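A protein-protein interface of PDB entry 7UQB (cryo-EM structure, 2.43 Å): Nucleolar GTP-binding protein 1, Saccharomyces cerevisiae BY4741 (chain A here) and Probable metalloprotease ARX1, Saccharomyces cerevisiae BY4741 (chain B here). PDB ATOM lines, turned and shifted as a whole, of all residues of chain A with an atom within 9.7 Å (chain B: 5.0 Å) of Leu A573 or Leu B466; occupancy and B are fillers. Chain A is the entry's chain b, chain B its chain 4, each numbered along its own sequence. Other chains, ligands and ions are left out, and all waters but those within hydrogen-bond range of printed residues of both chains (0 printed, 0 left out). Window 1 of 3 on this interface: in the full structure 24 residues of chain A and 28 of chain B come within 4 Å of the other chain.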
ATOM      1  N   VAL A 566       8.695  -8.421   1.374  1.00  0.00           N
ATOM      2  CA  VAL A 566       8.472  -7.656   2.597  1.00  0.00           C
ATOM      3  C   VAL A 566       8.207  -6.184   2.294  1.00  0.00           C
ATOM      4  O   VAL A 566       7.195  -5.625   2.731  1.00  0.00           O
ATOM      5  CB  VAL A 566       9.661  -7.804   3.562  1.00  0.00           C
ATOM      6  CG1 VAL A 566       9.400  -7.029   4.845  1.00  0.00           C
ATOM      7  CG2 VAL A 566       9.915  -9.270   3.867  1.00  0.00           C
ATOM      8  N   PHE A 567       9.110  -5.546   1.549  1.00  0.00           N
ATOM      9  CA  PHE A 567       9.076  -4.108   1.328  1.00  0.00           C
ATOM     10  C   PHE A 567       8.459  -3.719  -0.009  1.00  0.00           C
ATOM     11  O   PHE A 567       8.574  -2.559  -0.414  1.00  0.00           O
ATOM     12  CB  PHE A 567      10.491  -3.529   1.420  1.00  0.00           C
ATOM     13  CG  PHE A 567      11.111  -3.651   2.780  1.00  0.00           C
ATOM     14  CD1 PHE A 567      11.815  -4.789   3.137  1.00  0.00           C
ATOM     15  CD2 PHE A 567      11.002  -2.621   3.698  1.00  0.00           C
ATOM     16  CE1 PHE A 567      12.389  -4.901   4.386  1.00  0.00           C
ATOM     17  CE2 PHE A 567      11.574  -2.727   4.948  1.00  0.00           C
ATOM     18  CZ  PHE A 567      12.268  -3.867   5.293  1.00  0.00           C
ATOM     19  N   ASP A 569       5.234  -3.497  -1.103  1.00  0.00           N
ATOM     20  CA  ASP A 569       4.069  -2.626  -1.036  1.00  0.00           C
ATOM     21  C   ASP A 569       4.154  -1.588   0.075  1.00  0.00           C
ATOM     22  O   ASP A 569       3.176  -0.869   0.305  1.00  0.00           O
ATOM     23  CB  ASP A 569       2.797  -3.464  -0.862  1.00  0.00           C
ATOM     24  CG  ASP A 569       2.912  -4.470   0.266  1.00  0.00           C
ATOM     25  OD1 ASP A 569       3.982  -4.533   0.908  1.00  0.00           O
ATOM     26  OD2 ASP A 569       1.930  -5.201   0.506  1.00  0.00           O
ATOM     27  N   GLN A 570       5.281  -1.491   0.769  1.00  0.00           N
ATOM     28  CA  GLN A 570       5.431  -0.565   1.876  1.00  0.00           C
ATOM     29  C   GLN A 570       6.327   0.601   1.472  1.00  0.00           C
ATOM     30  O   GLN A 570       6.819   0.685   0.344  1.00  0.00           O
ATOM     31  CB  GLN A 570       5.987  -1.288   3.104  1.00  0.00           C
ATOM     32  CG  GLN A 570       5.056  -2.347   3.659  1.00  0.00           C
ATOM     33  CD  GLN A 570       5.632  -3.053   4.868  1.00  0.00           C
ATOM     34  OE1 GLN A 570       6.802  -2.876   5.207  1.00  0.00           O
ATOM     35  NE2 GLN A 570       4.808  -3.858   5.528  1.00  0.00           N
ATOM     36  N   ASP A 571       6.538   1.514   2.412  1.00  0.00           N
ATOM     37  CA  ASP A 571       7.393   2.671   2.186  1.00  0.00           C
ATOM     38  C   ASP A 571       7.898   3.160   3.539  1.00  0.00           C
ATOM     39  O   ASP A 571       7.716   2.494   4.564  1.00  0.00           O
ATOM     40  CB  ASP A 571       6.639   3.767   1.427  1.00  0.00           C
ATOM     41  CG  ASP A 571       7.535   4.546   0.486  1.00  0.00           C
ATOM     42  OD1 ASP A 571       8.595   4.012   0.098  1.00  0.00           O
ATOM     43  OD2 ASP A 571       7.183   5.692   0.138  1.00  0.00           O
ATOM     44  N   ALA A 572       8.558   4.320   3.528  1.00  0.00           N
ATOM     45  CA  ALA A 572       8.899   5.079   4.727  1.00  0.00           C
ATOM     46  C   ALA A 572       9.789   4.312   5.696  1.00  0.00           C
ATOM     47  O   ALA A 572      11.016   4.346   5.568  1.00  0.00           O
ATOM     48  CB  ALA A 572       7.626   5.541   5.446  1.00  0.00           C
ATOM     49  N   LEU A 573       9.173   3.674   6.694  1.00  0.00           N
ATOM     50  CA  LEU A 573       9.784   3.005   7.844  1.00  0.00           C
ATOM     51  C   LEU A 573      10.456   3.984   8.797  1.00  0.00           C
ATOM     52  O   LEU A 573      10.938   3.568   9.854  1.00  0.00           O
ATOM     53  CB  LEU A 573      10.805   1.929   7.447  1.00  0.00           C
ATOM     54  CG  LEU A 573      10.731   0.621   8.227  1.00  0.00           C
ATOM     55  CD1 LEU A 573       9.464  -0.125   7.843  1.00  0.00           C
ATOM     56  CD2 LEU A 573      11.964  -0.232   7.985  1.00  0.00           C
ATOM     57  N   THR A 574      10.489   5.271   8.467  1.00  0.00           N
ATOM     58  CA  THR A 574      11.160   6.281   9.269  1.00  0.00           C
ATOM     59  C   THR A 574      10.347   7.560   9.163  1.00  0.00           C
ATOM     60  O   THR A 574       9.918   7.926   8.064  1.00  0.00           O
ATOM     61  CB  THR A 574      12.602   6.495   8.785  1.00  0.00           C
ATOM     62  OG1 THR A 574      13.466   5.533   9.404  1.00  0.00           O
ATOM     63  CG2 THR A 574      13.093   7.897   9.098  1.00  0.00           C
ATOM     64  N   ALA A 575      10.111   8.212  10.302  1.00  0.00           N
ATOM     65  CA  ALA A 575       9.366   9.462  10.308  1.00  0.00           C
ATOM     66  C   ALA A 575      10.089  10.519   9.485  1.00  0.00           C
ATOM     67  O   ALA A 575      11.300  10.719   9.629  1.00  0.00           O
ATOM     68  CB  ALA A 575       9.168   9.950  11.742  1.00  0.00           C
ATOM     69  N   SER A 576       9.345  11.188   8.610  1.00  0.00           N
ATOM     70  CA  SER A 576       9.911  12.246   7.786  1.00  0.00           C
ATOM     71  C   SER A 576      10.050  13.517   8.611  1.00  0.00           C
ATOM     72  O   SER A 576       9.104  13.941   9.283  1.00  0.00           O
ATOM     73  CB  SER A 576       9.032  12.496   6.561  1.00  0.00           C
ATOM     74  OG  SER A 576       7.685  12.719   6.938  1.00  0.00           O
ATOM     75  N   THR A 577      11.235  14.119   8.565  1.00  0.00           N
ATOM     76  CA  THR A 577      11.500  15.323   9.335  1.00  0.00           C
ATOM     77  C   THR A 577      10.787  16.524   8.718  1.00  0.00           C
ATOM     78  O   THR A 577      10.474  16.555   7.525  1.00  0.00           O
ATOM     79  CB  THR A 577      13.004  15.586   9.411  1.00  0.00           C
ATOM     80  OG1 THR A 577      13.518  15.795   8.091  1.00  0.00           O
ATOM     81  CG2 THR A 577      13.716  14.399  10.037  1.00  0.00           C
ATOM     82  N   LEU A 583      19.974  12.342   9.797  1.00  0.00           N
ATOM     83  CA  LEU A 583      19.845  11.785  11.141  1.00  0.00           C
ATOM     84  C   LEU A 583      20.624  12.598  12.171  1.00  0.00           C
ATOM     85  O   LEU A 583      20.119  12.866  13.266  1.00  0.00           O
ATOM     86  CB  LEU A 583      20.314  10.331  11.145  1.00  0.00           C
ATOM     87  CG  LEU A 583      20.274   9.593  12.484  1.00  0.00           C
ATOM     88  CD1 LEU A 583      18.841   9.331  12.902  1.00  0.00           C
ATOM     89  CD2 LEU A 583      21.065   8.298  12.414  1.00  0.00           C
ATOM     90  N   ILE B 258       9.735  -2.682  14.111  1.00  0.00           N
ATOM     91  CA  ILE B 258      10.384  -1.771  13.178  1.00  0.00           C
ATOM     92  C   ILE B 258       9.666  -1.750  11.833  1.00  0.00           C
ATOM     93  O   ILE B 258       9.330  -0.687  11.313  1.00  0.00           O
ATOM     94  CB  ILE B 258      11.875  -2.134  13.004  1.00  0.00           C
ATOM     95  CG1 ILE B 258      12.540  -2.305  14.371  1.00  0.00           C
ATOM     96  CG2 ILE B 258      12.588  -1.074  12.187  1.00  0.00           C
ATOM     97  CD1 ILE B 258      13.993  -2.711  14.302  1.00  0.00           C
ATOM     98  N   VAL B 259       9.423  -2.923  11.258  1.00  0.00           N
ATOM     99  CA  VAL B 259       8.780  -3.047   9.956  1.00  0.00           C
ATOM    100  C   VAL B 259       7.310  -3.375  10.168  1.00  0.00           C
ATOM    101  O   VAL B 259       6.974  -4.324  10.886  1.00  0.00           O
ATOM    102  CB  VAL B 259       9.468  -4.121   9.095  1.00  0.00           C
ATOM    103  CG1 VAL B 259       8.792  -4.233   7.736  1.00  0.00           C
ATOM    104  CG2 VAL B 259      10.947  -3.802   8.933  1.00  0.00           C
ATOM    105  N   ALA B 260       6.435  -2.582   9.556  1.00  0.00           N
ATOM    106  CA  ALA B 260       5.010  -2.872   9.599  1.00  0.00           C
ATOM    107  C   ALA B 260       4.692  -4.072   8.714  1.00  0.00           C
ATOM    108  O   ALA B 260       5.415  -4.381   7.764  1.00  0.00           O
ATOM    109  CB  ALA B 260       4.202  -1.656   9.149  1.00  0.00           C
ATOM    110  N   ASP B 363      16.246  -0.939   5.364  1.00  0.00           N
ATOM    111  CA  ASP B 363      14.945  -0.485   4.881  1.00  0.00           C
ATOM    112  C   ASP B 363      15.007  -0.454   3.357  1.00  0.00           C
ATOM    113  O   ASP B 363      15.560   0.477   2.768  1.00  0.00           O
ATOM    114  CB  ASP B 363      14.604   0.883   5.459  1.00  0.00           C
ATOM    115  CG  ASP B 363      13.243   1.370   5.029  1.00  0.00           C
ATOM    116  OD1 ASP B 363      12.369   0.529   4.734  1.00  0.00           O
ATOM    117  OD2 ASP B 363      13.051   2.597   4.975  1.00  0.00           O
ATOM    118  N   VAL B 433      18.493   1.018  10.024  1.00  0.00           N
ATOM    119  CA  VAL B 433      18.164   1.463  11.368  1.00  0.00           C
ATOM    120  C   VAL B 433      18.683   0.444  12.371  1.00  0.00           C
ATOM    121  O   VAL B 433      18.941  -0.716  12.043  1.00  0.00           O
ATOM    122  CB  VAL B 433      16.650   1.685  11.560  1.00  0.00           C
ATOM    123  CG1 VAL B 433      16.193   2.909  10.784  1.00  0.00           C
ATOM    124  CG2 VAL B 433      15.877   0.453  11.133  1.00  0.00           C
ATOM    125  N   GLU B 434      18.841   0.902  13.607  1.00  0.00           N
ATOM    126  CA  GLU B 434      19.313   0.046  14.684  1.00  0.00           C
ATOM    127  C   GLU B 434      18.179  -0.808  15.236  1.00  0.00           C
ATOM    128  O   GLU B 434      17.009  -0.415  15.220  1.00  0.00           O
ATOM    129  CB  GLU B 434      19.913   0.887  15.808  1.00  0.00           C
ATOM    130  CG  GLU B 434      21.151   1.675  15.420  1.00  0.00           C
ATOM    131  CD  GLU B 434      21.577   2.651  16.499  1.00  0.00           C
ATOM    132  OE1 GLU B 434      20.691   3.207  17.181  1.00  0.00           O
ATOM    133  OE2 GLU B 434      22.797   2.857  16.672  1.00  0.00           O
ATOM    134  N   SER B 464      11.822  10.946  17.582  1.00  0.00           N
ATOM    135  CA  SER B 464      11.979   9.513  17.370  1.00  0.00           C
ATOM    136  C   SER B 464      12.331   9.217  15.918  1.00  0.00           C
ATOM    137  O   SER B 464      11.777   9.814  14.991  1.00  0.00           O
ATOM    138  CB  SER B 464      10.699   8.779  17.762  1.00  0.00           C
ATOM    139  OG  SER B 464      10.825   7.384  17.555  1.00  0.00           O
ATOM    140  N   THR B 465      13.270   8.291  15.725  1.00  0.00           N
ATOM    141  CA  THR B 465      13.770   8.003  14.388  1.00  0.00           C
ATOM    142  C   THR B 465      12.896   6.999  13.645  1.00  0.00           C
ATOM    143  O   THR B 465      12.860   7.014  12.411  1.00  0.00           O
ATOM    144  CB  THR B 465      15.210   7.494  14.469  1.00  0.00           C
ATOM    145  OG1 THR B 465      15.242   6.255  15.187  1.00  0.00           O
ATOM    146  CG2 THR B 465      16.083   8.502  15.199  1.00  0.00           C
ATOM    147  N   LEU B 466      12.190   6.132  14.366  1.00  0.00           N
ATOM    148  CA  LEU B 466      11.321   5.131  13.762  1.00  0.00           C
ATOM    149  C   LEU B 466       9.861   5.546  13.898  1.00  0.00           C
ATOM    150  O   LEU B 466       9.458   6.121  14.914  1.00  0.00           O
ATOM    151  CB  LEU B 466      11.533   3.759  14.405  1.00  0.00           C
ATOM    152  CG  LEU B 466      12.707   2.886  13.950  1.00  0.00           C
ATOM    153  CD1 LEU B 466      12.809   2.874  12.435  1.00  0.00           C
ATOM    154  CD2 LEU B 466      14.018   3.321  14.586  1.00  0.00           C
ATOM    155  N   THR B 467       9.071   5.249  12.863  1.00  0.00           N
ATOM    156  CA  THR B 467       7.668   5.653  12.852  1.00  0.00           C
ATOM    157  C   THR B 467       6.845   4.851  13.856  1.00  0.00           C
ATOM    158  O   THR B 467       6.051   5.421  14.616  1.00  0.00           O
ATOM    159  CB  THR B 467       7.089   5.500  11.444  1.00  0.00           C
ATOM    160  OG1 THR B 467       7.716   6.439  10.562  1.00  0.00           O
ATOM    161  CG2 THR B 467       5.584   5.741  11.447  1.00  0.00           C
ATOM    162  N   LEU B 468       7.018   3.528  13.871  1.00  0.00           N
ATOM    163  CA  LEU B 468       6.148   2.665  14.672  1.00  0.00           C
ATOM    164  C   LEU B 468       6.237   2.928  16.173  1.00  0.00           C
ATOM    165  O   LEU B 468       5.178   3.067  16.808  1.00  0.00           O
ATOM    166  CB  LEU B 468       6.425   1.193  14.331  1.00  0.00           C
ATOM    167  CG  LEU B 468       5.562   0.497  13.272  1.00  0.00           C
ATOM    168  CD1 LEU B 468       5.456   1.318  12.000  1.00  0.00           C
ATOM    169  CD2 LEU B 468       6.128  -0.885  12.969  1.00  0.00           C
ATOM    170  N   PRO B 469       7.417   3.014  16.809  1.00  0.00           N
ATOM    171  CA  PRO B 469       7.431   3.375  18.234  1.00  0.00           C
ATOM    172  C   PRO B 469       7.221   4.855  18.493  1.00  0.00           C
ATOM    173  O   PRO B 469       6.801   5.212  19.602  1.00  0.00           O
ATOM    174  CB  PRO B 469       8.830   2.934  18.703  1.00  0.00           C
ATOM    175  CG  PRO B 469       9.387   2.103  17.592  1.00  0.00           C
ATOM    176  CD  PRO B 469       8.775   2.657  16.359  1.00  0.00           C
ATOM    177  N   GLY B 470       7.500   5.719  17.515  1.00  0.00           N
ATOM    178  CA  GLY B 470       7.385   7.151  17.744  1.00  0.00           C
ATOM    179  C   GLY B 470       5.956   7.605  17.978  1.00  0.00           C
ATOM    180  O   GLY B 470       5.702   8.485  18.804  1.00  0.00           O
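Among the printed residues, merely in contact across the chains: Thr A574 with Thr B467 (3.2 Å), Leu A573 with Leu B466 (3.3 Å), Phe A567 with Asp B363 (3.4 Å), Leu A573 with Asp B363 (3.4 Å), Gln A570 with Val B259 (3.5 Å), Leu A573 with Ile B258 (3.5 Å), Ala A575 with Thr B465 (3.7 Å), Leu A573 with Val B259 (3.7 Å), Leu A583 with Thr B465 (3.7 Å), Phe A567 with Val B259 (3.9 Å) and Leu A573 with Thr B467 (3.9 Å).
O of Leu B466 sits at hydrogen-bond distance from OG of Ser B464, 3.2 Å away.
The backbone carbonyl oxygen (O) of Ala A572 lies close to the side-chain carboxylate (OD2) of Asp B363 (2.7 Å). The backbone NH (N) of Ala A575 sits at hydrogen-bond distance from the side-chain hydroxyl (OG1) of Thr B467 (3.0 Å). The backbone carbonyl oxygen of Ala B260 sits close to the side-chain amide oxygen of Gln A570 (3.3 Å). The side-chain hydroxyl of Thr A574 is in hydrogen-bond range of the backbone carbonyl oxygen of Thr B465 (3.4 Å).
Of the 12 printed residues of chain A, 7 touch a printed residue of chain B. Printed residues of chain A that touch a printed residue of chain B: Phe A567, Gln A570, Ala A572, Leu A573, Thr A574, Ala A575 and Leu A583. Hydrophobic or aromatic side chains of chain A within 4 Å of the printed part of chain B: Phe A567, Leu A573, Ala A575 and Leu A583. Of the 13 printed residues of chain B, 7 touch a printed residue of chain A. Printed residues of chain B that touch a printed residue of chain A: Ile B258, Val B259, Ala B260, Asp B363, Thr B465, Leu B466 and Thr B467. Hydrophobic or aromatic side chains of chain B within 4 Å of the printed part of chain A: Val B259 and Leu B466. Along chain B the printed residues that touch a printed residue of chain A span positions 258 to 467. Among the printed residues, 15 pairs touch across the chains.
Of the printed residues of chain B, Leu A573 touches Ile B258 (3.5 Å), Val B259 (3.7 Å), Asp B363 (3.4 Å), Leu B466 (3.3 Å) and Thr B467 (3.9 Å). Leu B466 touches just one residue of chain A: Leu A573 (3.3 Å). Thr B465 touches just these residues of chain A: Thr A574 (3.4 Å), Ala A575 (3.7 Å) and Leu A583 (3.7 Å). No residue of chain A comes within 4 Å of Pro B469. Of the printed residues of chain A, Ala B260 touches Gln A570 (2.4 Å). Printed residues of chain B within 4 Å of Leu A583: Thr B465. Val A566 touches none of the printed residues of chain B. The nearest residue of chain A that does not touch Leu B466 is Thr A574 (4.1 Å). The nearest printed residue of chain B that does not touch Ala A572 is Thr B467 (5.2 Å).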
